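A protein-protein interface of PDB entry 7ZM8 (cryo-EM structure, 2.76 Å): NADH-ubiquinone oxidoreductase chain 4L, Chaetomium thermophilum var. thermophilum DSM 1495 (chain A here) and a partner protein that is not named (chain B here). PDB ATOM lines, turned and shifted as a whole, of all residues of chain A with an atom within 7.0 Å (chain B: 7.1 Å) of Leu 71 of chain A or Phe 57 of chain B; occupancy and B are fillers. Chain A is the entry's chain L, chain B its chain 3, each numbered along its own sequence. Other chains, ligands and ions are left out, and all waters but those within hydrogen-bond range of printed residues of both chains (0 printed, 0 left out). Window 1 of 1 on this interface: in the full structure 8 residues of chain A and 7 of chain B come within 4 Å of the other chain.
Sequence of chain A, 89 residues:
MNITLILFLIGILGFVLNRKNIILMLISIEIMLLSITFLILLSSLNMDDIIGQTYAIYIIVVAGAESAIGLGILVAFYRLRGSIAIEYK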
ATOM      1  N   ILE A  23     -22.042  38.456  -5.830  1.00  0.00           N
ATOM      2  CA  ILE A  23     -21.496  37.115  -6.001  1.00  0.00           C
ATOM      3  C   ILE A  23     -19.979  37.146  -5.890  1.00  0.00           C
ATOM      4  O   ILE A  23     -19.371  36.269  -5.270  1.00  0.00           O
ATOM      5  CB  ILE A  23     -21.952  36.521  -7.345  1.00  0.00           C
ATOM      6  CG1 ILE A  23     -23.462  36.311  -7.355  1.00  0.00           C
ATOM      7  CG2 ILE A  23     -21.261  35.194  -7.606  1.00  0.00           C
ATOM      8  CD1 ILE A  23     -23.928  35.316  -6.343  1.00  0.00           C
ATOM      9  N   LEU A  26     -18.722  36.978  -2.440  1.00  0.00           N
ATOM     10  CA  LEU A  26     -18.648  35.600  -1.967  1.00  0.00           C
ATOM     11  C   LEU A  26     -17.382  34.921  -2.459  1.00  0.00           C
ATOM     12  O   LEU A  26     -16.739  34.174  -1.716  1.00  0.00           O
ATOM     13  CB  LEU A  26     -19.872  34.806  -2.419  1.00  0.00           C
ATOM     14  CG  LEU A  26     -21.120  34.859  -1.544  1.00  0.00           C
ATOM     15  CD1 LEU A  26     -20.796  34.245  -0.201  1.00  0.00           C
ATOM     16  CD2 LEU A  26     -21.646  36.253  -1.382  1.00  0.00           C
ATOM     17  N   ALA A  65     -19.177  25.541   5.322  1.00  0.00           N
ATOM     18  CA  ALA A  65     -20.393  25.838   6.111  1.00  0.00           C
ATOM     19  C   ALA A  65     -20.815  27.284   5.874  1.00  0.00           C
ATOM     20  O   ALA A  65     -22.010  27.527   5.770  1.00  0.00           O
ATOM     21  CB  ALA A  65     -20.139  25.552   7.563  1.00  0.00           C
ATOM     22  N   GLU A  66     -19.881  28.229   5.791  1.00  0.00           N
ATOM     23  CA  GLU A  66     -20.292  29.624   5.477  1.00  0.00           C
ATOM     24  C   GLU A  66     -20.802  29.716   4.043  1.00  0.00           C
ATOM     25  O   GLU A  66     -21.694  30.528   3.801  1.00  0.00           O
ATOM     26  CB  GLU A  66     -19.197  30.655   5.748  1.00  0.00           C
ATOM     27  CG  GLU A  66     -18.050  30.686   4.766  1.00  0.00           C
ATOM     28  CD  GLU A  66     -16.953  31.630   5.217  1.00  0.00           C
ATOM     29  OE1 GLU A  66     -16.084  31.194   5.999  1.00  0.00           O
ATOM     30  OE2 GLU A  66     -16.986  32.805   4.810  1.00  0.00           O
ATOM     31  N   SER A  67     -20.238  28.924   3.135  1.00  0.00           N
ATOM     32  CA  SER A  67     -20.734  28.914   1.746  1.00  0.00           C
ATOM     33  C   SER A  67     -22.186  28.456   1.723  1.00  0.00           C
ATOM     34  O   SER A  67     -22.987  29.081   1.024  1.00  0.00           O
ATOM     35  CB  SER A  67     -19.880  27.992   0.975  1.00  0.00           C
ATOM     36  OG  SER A  67     -18.514  28.359   1.091  1.00  0.00           O
ATOM     37  N   ALA A  68     -22.510  27.421   2.480  1.00  0.00           N
ATOM     38  CA  ALA A  68     -23.898  26.938   2.572  1.00  0.00           C
ATOM     39  C   ALA A  68     -24.793  27.995   3.206  1.00  0.00           C
ATOM     40  O   ALA A  68     -25.870  28.247   2.661  1.00  0.00           O
ATOM     41  CB  ALA A  68     -23.886  25.708   3.444  1.00  0.00           C
ATOM     42  N   ILE A  69     -24.354  28.579   4.317  1.00  0.00           N
ATOM     43  CA  ILE A  69     -25.170  29.589   5.046  1.00  0.00           C
ATOM     44  C   ILE A  69     -25.332  30.823   4.154  1.00  0.00           C
ATOM     45  O   ILE A  69     -26.414  31.391   4.144  1.00  0.00           O
ATOM     46  CB  ILE A  69     -24.550  29.863   6.433  1.00  0.00           C
ATOM     47  CG1 ILE A  69     -24.815  28.706   7.396  1.00  0.00           C
ATOM     48  CG2 ILE A  69     -25.036  31.183   7.017  1.00  0.00           C
ATOM     49  CD1 ILE A  69     -26.273  28.360   7.518  1.00  0.00           C
ATOM     50  N   GLY A  70     -24.274  31.222   3.453  1.00  0.00           N
ATOM     51  CA  GLY A  70     -24.311  32.382   2.556  1.00  0.00           C
ATOM     52  C   GLY A  70     -25.161  32.211   1.326  1.00  0.00           C
ATOM     53  O   GLY A  70     -25.823  33.183   0.959  1.00  0.00           O
ATOM     54  N   LEU A  71     -25.090  31.048   0.673  1.00  0.00           N
ATOM     55  CA  LEU A  71     -25.827  30.877  -0.596  1.00  0.00           C
ATOM     56  C   LEU A  71     -27.275  30.601  -0.234  1.00  0.00           C
ATOM     57  O   LEU A  71     -28.136  30.886  -1.060  1.00  0.00           O
ATOM     58  CB  LEU A  71     -25.185  29.785  -1.449  1.00  0.00           C
ATOM     59  CG  LEU A  71     -23.900  30.179  -2.173  1.00  0.00           C
ATOM     60  CD1 LEU A  71     -23.310  28.988  -2.909  1.00  0.00           C
ATOM     61  CD2 LEU A  71     -24.151  31.326  -3.135  1.00  0.00           C
ATOM     62  N   GLY A  72     -27.522  30.100   0.975  1.00  0.00           N
ATOM     63  CA  GLY A  72     -28.904  29.989   1.398  1.00  0.00           C
ATOM     64  C   GLY A  72     -29.552  31.334   1.651  1.00  0.00           C
ATOM     65  O   GLY A  72     -30.715  31.548   1.300  1.00  0.00           O
ATOM     66  N   ILE A  73     -28.818  32.251   2.282  1.00  0.00           N
ATOM     67  CA  ILE A  73     -29.340  33.592   2.513  1.00  0.00           C
ATOM     68  C   ILE A  73     -29.509  34.325   1.191  1.00  0.00           C
ATOM     69  O   ILE A  73     -30.457  35.096   1.006  1.00  0.00           O
ATOM     70  CB  ILE A  73     -28.423  34.359   3.485  1.00  0.00           C
ATOM     71  CG1 ILE A  73     -28.535  33.774   4.889  1.00  0.00           C
ATOM     72  CG2 ILE A  73     -28.768  35.835   3.526  1.00  0.00           C
ATOM     73  CD1 ILE A  73     -27.611  34.409   5.891  1.00  0.00           C
ATOM     74  N   LEU A  74     -28.594  34.098   0.250  1.00  0.00           N
ATOM     75  CA  LEU A  74     -28.729  34.700  -1.069  1.00  0.00           C
ATOM     76  C   LEU A  74     -29.963  34.175  -1.794  1.00  0.00           C
ATOM     77  O   LEU A  74     -30.572  34.891  -2.594  1.00  0.00           O
ATOM     78  CB  LEU A  74     -27.466  34.436  -1.884  1.00  0.00           C
ATOM     79  CG  LEU A  74     -27.454  34.994  -3.300  1.00  0.00           C
ATOM     80  CD1 LEU A  74     -27.022  36.438  -3.293  1.00  0.00           C
ATOM     81  CD2 LEU A  74     -26.555  34.160  -4.183  1.00  0.00           C
ATOM     82  N   VAL A  75     -30.336  32.921  -1.544  1.00  0.00           N
ATOM     83  CA  VAL A  75     -31.551  32.378  -2.141  1.00  0.00           C
ATOM     84  C   VAL A  75     -32.782  33.011  -1.513  1.00  0.00           C
ATOM     85  O   VAL A  75     -33.734  33.374  -2.211  1.00  0.00           O
ATOM     86  CB  VAL A  75     -31.571  30.844  -2.015  1.00  0.00           C
ATOM     87  CG1 VAL A  75     -32.956  30.307  -2.296  1.00  0.00           C
ATOM     88  CG2 VAL A  75     -30.573  30.230  -2.961  1.00  0.00           C
ATOM     89  N   ALA A  76     -32.771  33.205  -0.199  1.00  0.00           N
ATOM     90  CA  ALA A  76     -33.892  33.870   0.503  1.00  0.00           C
ATOM     91  C   ALA A  76     -34.068  35.293  -0.035  1.00  0.00           C
ATOM     92  O   ALA A  76     -35.228  35.716  -0.240  1.00  0.00           O
ATOM     93  CB  ALA A  76     -33.610  33.860   1.977  1.00  0.00           C
ATOM     94  N   PHE B  52     -36.999  28.990  -9.991  1.00  0.00           N
ATOM     95  CA  PHE B  52     -36.350  27.694  -9.917  1.00  0.00           C
ATOM     96  C   PHE B  52     -36.724  26.997  -8.616  1.00  0.00           C
ATOM     97  O   PHE B  52     -36.997  27.640  -7.599  1.00  0.00           O
ATOM     98  CB  PHE B  52     -34.827  27.826 -10.034  1.00  0.00           C
ATOM     99  CG  PHE B  52     -34.167  28.437  -8.831  1.00  0.00           C
ATOM    100  CD1 PHE B  52     -34.079  29.805  -8.697  1.00  0.00           C
ATOM    101  CD2 PHE B  52     -33.611  27.638  -7.849  1.00  0.00           C
ATOM    102  CE1 PHE B  52     -33.468  30.362  -7.607  1.00  0.00           C
ATOM    103  CE2 PHE B  52     -32.999  28.193  -6.750  1.00  0.00           C
ATOM    104  CZ  PHE B  52     -32.927  29.556  -6.629  1.00  0.00           C
ATOM    105  N   ASN B  53     -36.743  25.671  -8.662  1.00  0.00           N
ATOM    106  CA  ASN B  53     -37.128  24.886  -7.500  1.00  0.00           C
ATOM    107  C   ASN B  53     -36.074  24.977  -6.408  1.00  0.00           C
ATOM    108  O   ASN B  53     -34.872  24.893  -6.672  1.00  0.00           O
ATOM    109  CB  ASN B  53     -37.347  23.432  -7.896  1.00  0.00           C
ATOM    110  CG  ASN B  53     -38.406  23.277  -8.961  1.00  0.00           C
ATOM    111  OD1 ASN B  53     -39.590  23.512  -8.716  1.00  0.00           O
ATOM    112  ND2 ASN B  53     -37.988  22.887 -10.161  1.00  0.00           N
ATOM    113  N   ILE B  54     -36.536  25.140  -5.167  1.00  0.00           N
ATOM    114  CA  ILE B  54     -35.631  25.177  -4.030  1.00  0.00           C
ATOM    115  C   ILE B  54     -34.932  23.840  -3.830  1.00  0.00           C
ATOM    116  O   ILE B  54     -33.915  23.773  -3.137  1.00  0.00           O
ATOM    117  CB  ILE B  54     -36.405  25.616  -2.770  1.00  0.00           C
ATOM    118  CG1 ILE B  54     -35.443  25.953  -1.632  1.00  0.00           C
ATOM    119  CG2 ILE B  54     -37.374  24.533  -2.342  1.00  0.00           C
ATOM    120  CD1 ILE B  54     -34.525  27.086  -1.941  1.00  0.00           C
ATOM    121  N   SER B  55     -35.427  22.806  -4.475  1.00  0.00           N
ATOM    122  CA  SER B  55     -34.875  21.451  -4.281  1.00  0.00           C
ATOM    123  C   SER B  55     -33.430  21.405  -4.765  1.00  0.00           C
ATOM    124  O   SER B  55     -32.620  20.766  -4.086  1.00  0.00           O
ATOM    125  CB  SER B  55     -35.759  20.464  -4.982  1.00  0.00           C
ATOM    126  OG  SER B  55     -35.798  20.724  -6.377  1.00  0.00           O
ATOM    127  N   PHE B  56     -33.135  22.067  -5.883  1.00  0.00           N
ATOM    128  CA  PHE B  56     -31.758  22.106  -6.444  1.00  0.00           C
ATOM    129  C   PHE B  56     -30.767  22.642  -5.409  1.00  0.00           C
ATOM    130  O   PHE B  56     -29.648  22.113  -5.329  1.00  0.00           O
ATOM    131  CB  PHE B  56     -31.739  22.914  -7.741  1.00  0.00           C
ATOM    132  CG  PHE B  56     -32.341  22.202  -8.922  1.00  0.00           C
ATOM    133  CD1 PHE B  56     -31.773  21.037  -9.409  1.00  0.00           C
ATOM    134  CD2 PHE B  56     -33.472  22.697  -9.550  1.00  0.00           C
ATOM    135  CE1 PHE B  56     -32.325  20.381 -10.496  1.00  0.00           C
ATOM    136  CE2 PHE B  56     -34.023  22.040 -10.639  1.00  0.00           C
ATOM    137  CZ  PHE B  56     -33.447  20.885 -11.110  1.00  0.00           C
ATOM    138  N   PHE B  57     -31.164  23.665  -4.653  1.00  0.00           N
ATOM    139  CA  PHE B  57     -30.286  24.173  -3.608  1.00  0.00           C
ATOM    140  C   PHE B  57     -30.068  23.133  -2.521  1.00  0.00           C
ATOM    141  O   PHE B  57     -28.947  22.961  -2.032  1.00  0.00           O
ATOM    142  CB  PHE B  57     -30.857  25.461  -3.013  1.00  0.00           C
ATOM    143  CG  PHE B  57     -30.122  25.929  -1.798  1.00  0.00           C
ATOM    144  CD1 PHE B  57     -28.804  26.328  -1.883  1.00  0.00           C
ATOM    145  CD2 PHE B  57     -30.734  25.930  -0.562  1.00  0.00           C
ATOM    146  CE1 PHE B  57     -28.117  26.735  -0.760  1.00  0.00           C
ATOM    147  CE2 PHE B  57     -30.053  26.334   0.558  1.00  0.00           C
ATOM    148  CZ  PHE B  57     -28.743  26.735   0.459  1.00  0.00           C
ATOM    149  N   ILE B  58     -31.129  22.429  -2.134  1.00  0.00           N
ATOM    150  CA  ILE B  58     -31.056  21.506  -1.009  1.00  0.00           C
ATOM    151  C   ILE B  58     -30.163  20.318  -1.339  1.00  0.00           C
ATOM    152  O   ILE B  58     -29.457  19.797  -0.470  1.00  0.00           O
ATOM    153  CB  ILE B  58     -32.472  21.063  -0.605  1.00  0.00           C
ATOM    154  CG1 ILE B  58     -33.379  22.285  -0.442  1.00  0.00           C
ATOM    155  CG2 ILE B  58     -32.438  20.222   0.662  1.00  0.00           C
ATOM    156  CD1 ILE B  58     -32.851  23.318   0.495  1.00  0.00           C
ATOM    157  N   TYR B  59     -30.181  19.864  -2.591  1.00  0.00           N
ATOM    158  CA  TYR B  59     -29.355  18.726  -2.976  1.00  0.00           C
ATOM    159  C   TYR B  59     -27.875  19.038  -2.803  1.00  0.00           C
ATOM    160  O   TYR B  59     -27.112  18.215  -2.289  1.00  0.00           O
ATOM    161  CB  TYR B  59     -29.662  18.320  -4.416  1.00  0.00           C
ATOM    162  CG  TYR B  59     -31.010  17.664  -4.561  1.00  0.00           C
ATOM    163  CD1 TYR B  59     -31.499  16.834  -3.573  1.00  0.00           C
ATOM    164  CD2 TYR B  59     -31.797  17.883  -5.676  1.00  0.00           C
ATOM    165  CE1 TYR B  59     -32.730  16.238  -3.689  1.00  0.00           C
ATOM    166  CE2 TYR B  59     -33.033  17.285  -5.802  1.00  0.00           C
ATOM    167  CZ  TYR B  59     -33.491  16.464  -4.800  1.00  0.00           C
ATOM    168  OH  TYR B  59     -34.719  15.856  -4.905  1.00  0.00           O
ATOM    169  N   GLY B  60     -27.451  20.229  -3.222  1.00  0.00           N
ATOM    170  CA  GLY B  60     -26.065  20.611  -3.027  1.00  0.00           C
ATOM    171  C   GLY B  60     -25.744  20.973  -1.594  1.00  0.00           C
ATOM    172  O   GLY B  60     -24.616  20.777  -1.139  1.00  0.00           O
ATOM    173  N   LEU B  61     -26.719  21.516  -0.873  1.00  0.00           N
ATOM    174  CA  LEU B  61     -26.523  21.882   0.522  1.00  0.00           C
ATOM    175  C   LEU B  61     -26.261  20.657   1.382  1.00  0.00           C
ATOM    176  O   LEU B  61     -25.289  20.609   2.143  1.00  0.00           O
ATOM    177  CB  LEU B  61     -27.763  22.612   1.022  1.00  0.00           C
ATOM    178  CG  LEU B  61     -27.766  23.149   2.444  1.00  0.00           C
ATOM    179  CD1 LEU B  61     -26.701  24.199   2.618  1.00  0.00           C
ATOM    180  CD2 LEU B  61     -29.136  23.677   2.782  1.00  0.00           C
ATOM    181  N   VAL B  62     -27.137  19.660   1.288  1.00  0.00           N
ATOM    182  CA  VAL B  62     -27.012  18.481   2.127  1.00  0.00           C
ATOM    183  C   VAL B  62     -25.833  17.631   1.691  1.00  0.00           C
ATOM    184  O   VAL B  62     -25.172  17.002   2.524  1.00  0.00           O
ATOM    185  CB  VAL B  62     -28.331  17.696   2.114  1.00  0.00           C
ATOM    186  CG1 VAL B  62     -28.251  16.541   3.073  1.00  0.00           C
ATOM    187  CG2 VAL B  62     -29.476  18.616   2.489  1.00  0.00           C
ATOM    188  N   PHE B  63     -25.544  17.593   0.392  1.00  0.00           N
ATOM    189  CA  PHE B  63     -24.343  16.922  -0.078  1.00  0.00           C
ATOM    190  C   PHE B  63     -23.093  17.568   0.503  1.00  0.00           C
ATOM    191  O   PHE B  63     -22.205  16.877   1.007  1.00  0.00           O
ATOM    192  CB  PHE B  63     -24.305  16.945  -1.603  1.00  0.00           C
ATOM    193  CG  PHE B  63     -23.000  16.515  -2.186  1.00  0.00           C
ATOM    194  CD1 PHE B  63     -22.515  15.251  -1.967  1.00  0.00           C
ATOM    195  CD2 PHE B  63     -22.263  17.373  -2.961  1.00  0.00           C
ATOM    196  CE1 PHE B  63     -21.321  14.849  -2.502  1.00  0.00           C
ATOM    197  CE2 PHE B  63     -21.067  16.972  -3.501  1.00  0.00           C
ATOM    198  CZ  PHE B  63     -20.600  15.709  -3.273  1.00  0.00           C
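Among the printed residues, pairs that only touch across the chains: Ala 68 of chain A with Phe 57 of chain B (3.9 Å), Ala 68 of chain A with Leu 61 of chain B (3.3 Å), Leu 71 of chain A with Phe 57 of chain B (3.99 Å), Gly 72 of chain A with Phe 57 of chain B (3.4 Å) and Val 75 of chain A with Ile 54 of chain B (3.6 Å).
Of the 12 printed residues of chain B, 3 touch a printed residue of chain A.
Printed residues of chain B that touch a printed residue of chain A: Ile 54, Phe 57 and Leu 61.
Of the printed residues of chain A, Phe 57 of chain B touches Ala 68 (3.9 Å), Leu 71 (3.99 Å) and Gly 72 (3.4 Å).
Of the printed residues of chain A, Leu 61 of chain B touches Ala 68.
Printed residues of chain A within 4 Å of Ile 54 of chain B: Val 75 (3.6 Å).
Printed residues of chain B within 4 Å of Val 75 of chain A: Ile 54 (3.6 Å).
Printed residues of chain B within 4 Å of Ala 68 of chain A: Phe 57 and Leu 61.
Printed residues of chain B within 4 Å of Gly 72 of chain A: Phe 57 (3.4 Å).
Ala 65 of chain A touches none of the printed residues of chain B.
Ile 23 of chain A touches none of the printed residues of chain B.
The nearest printed residue of chain A that does not touch Phe 57 of chain B is Val 75 of chain A (4.4 Å).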
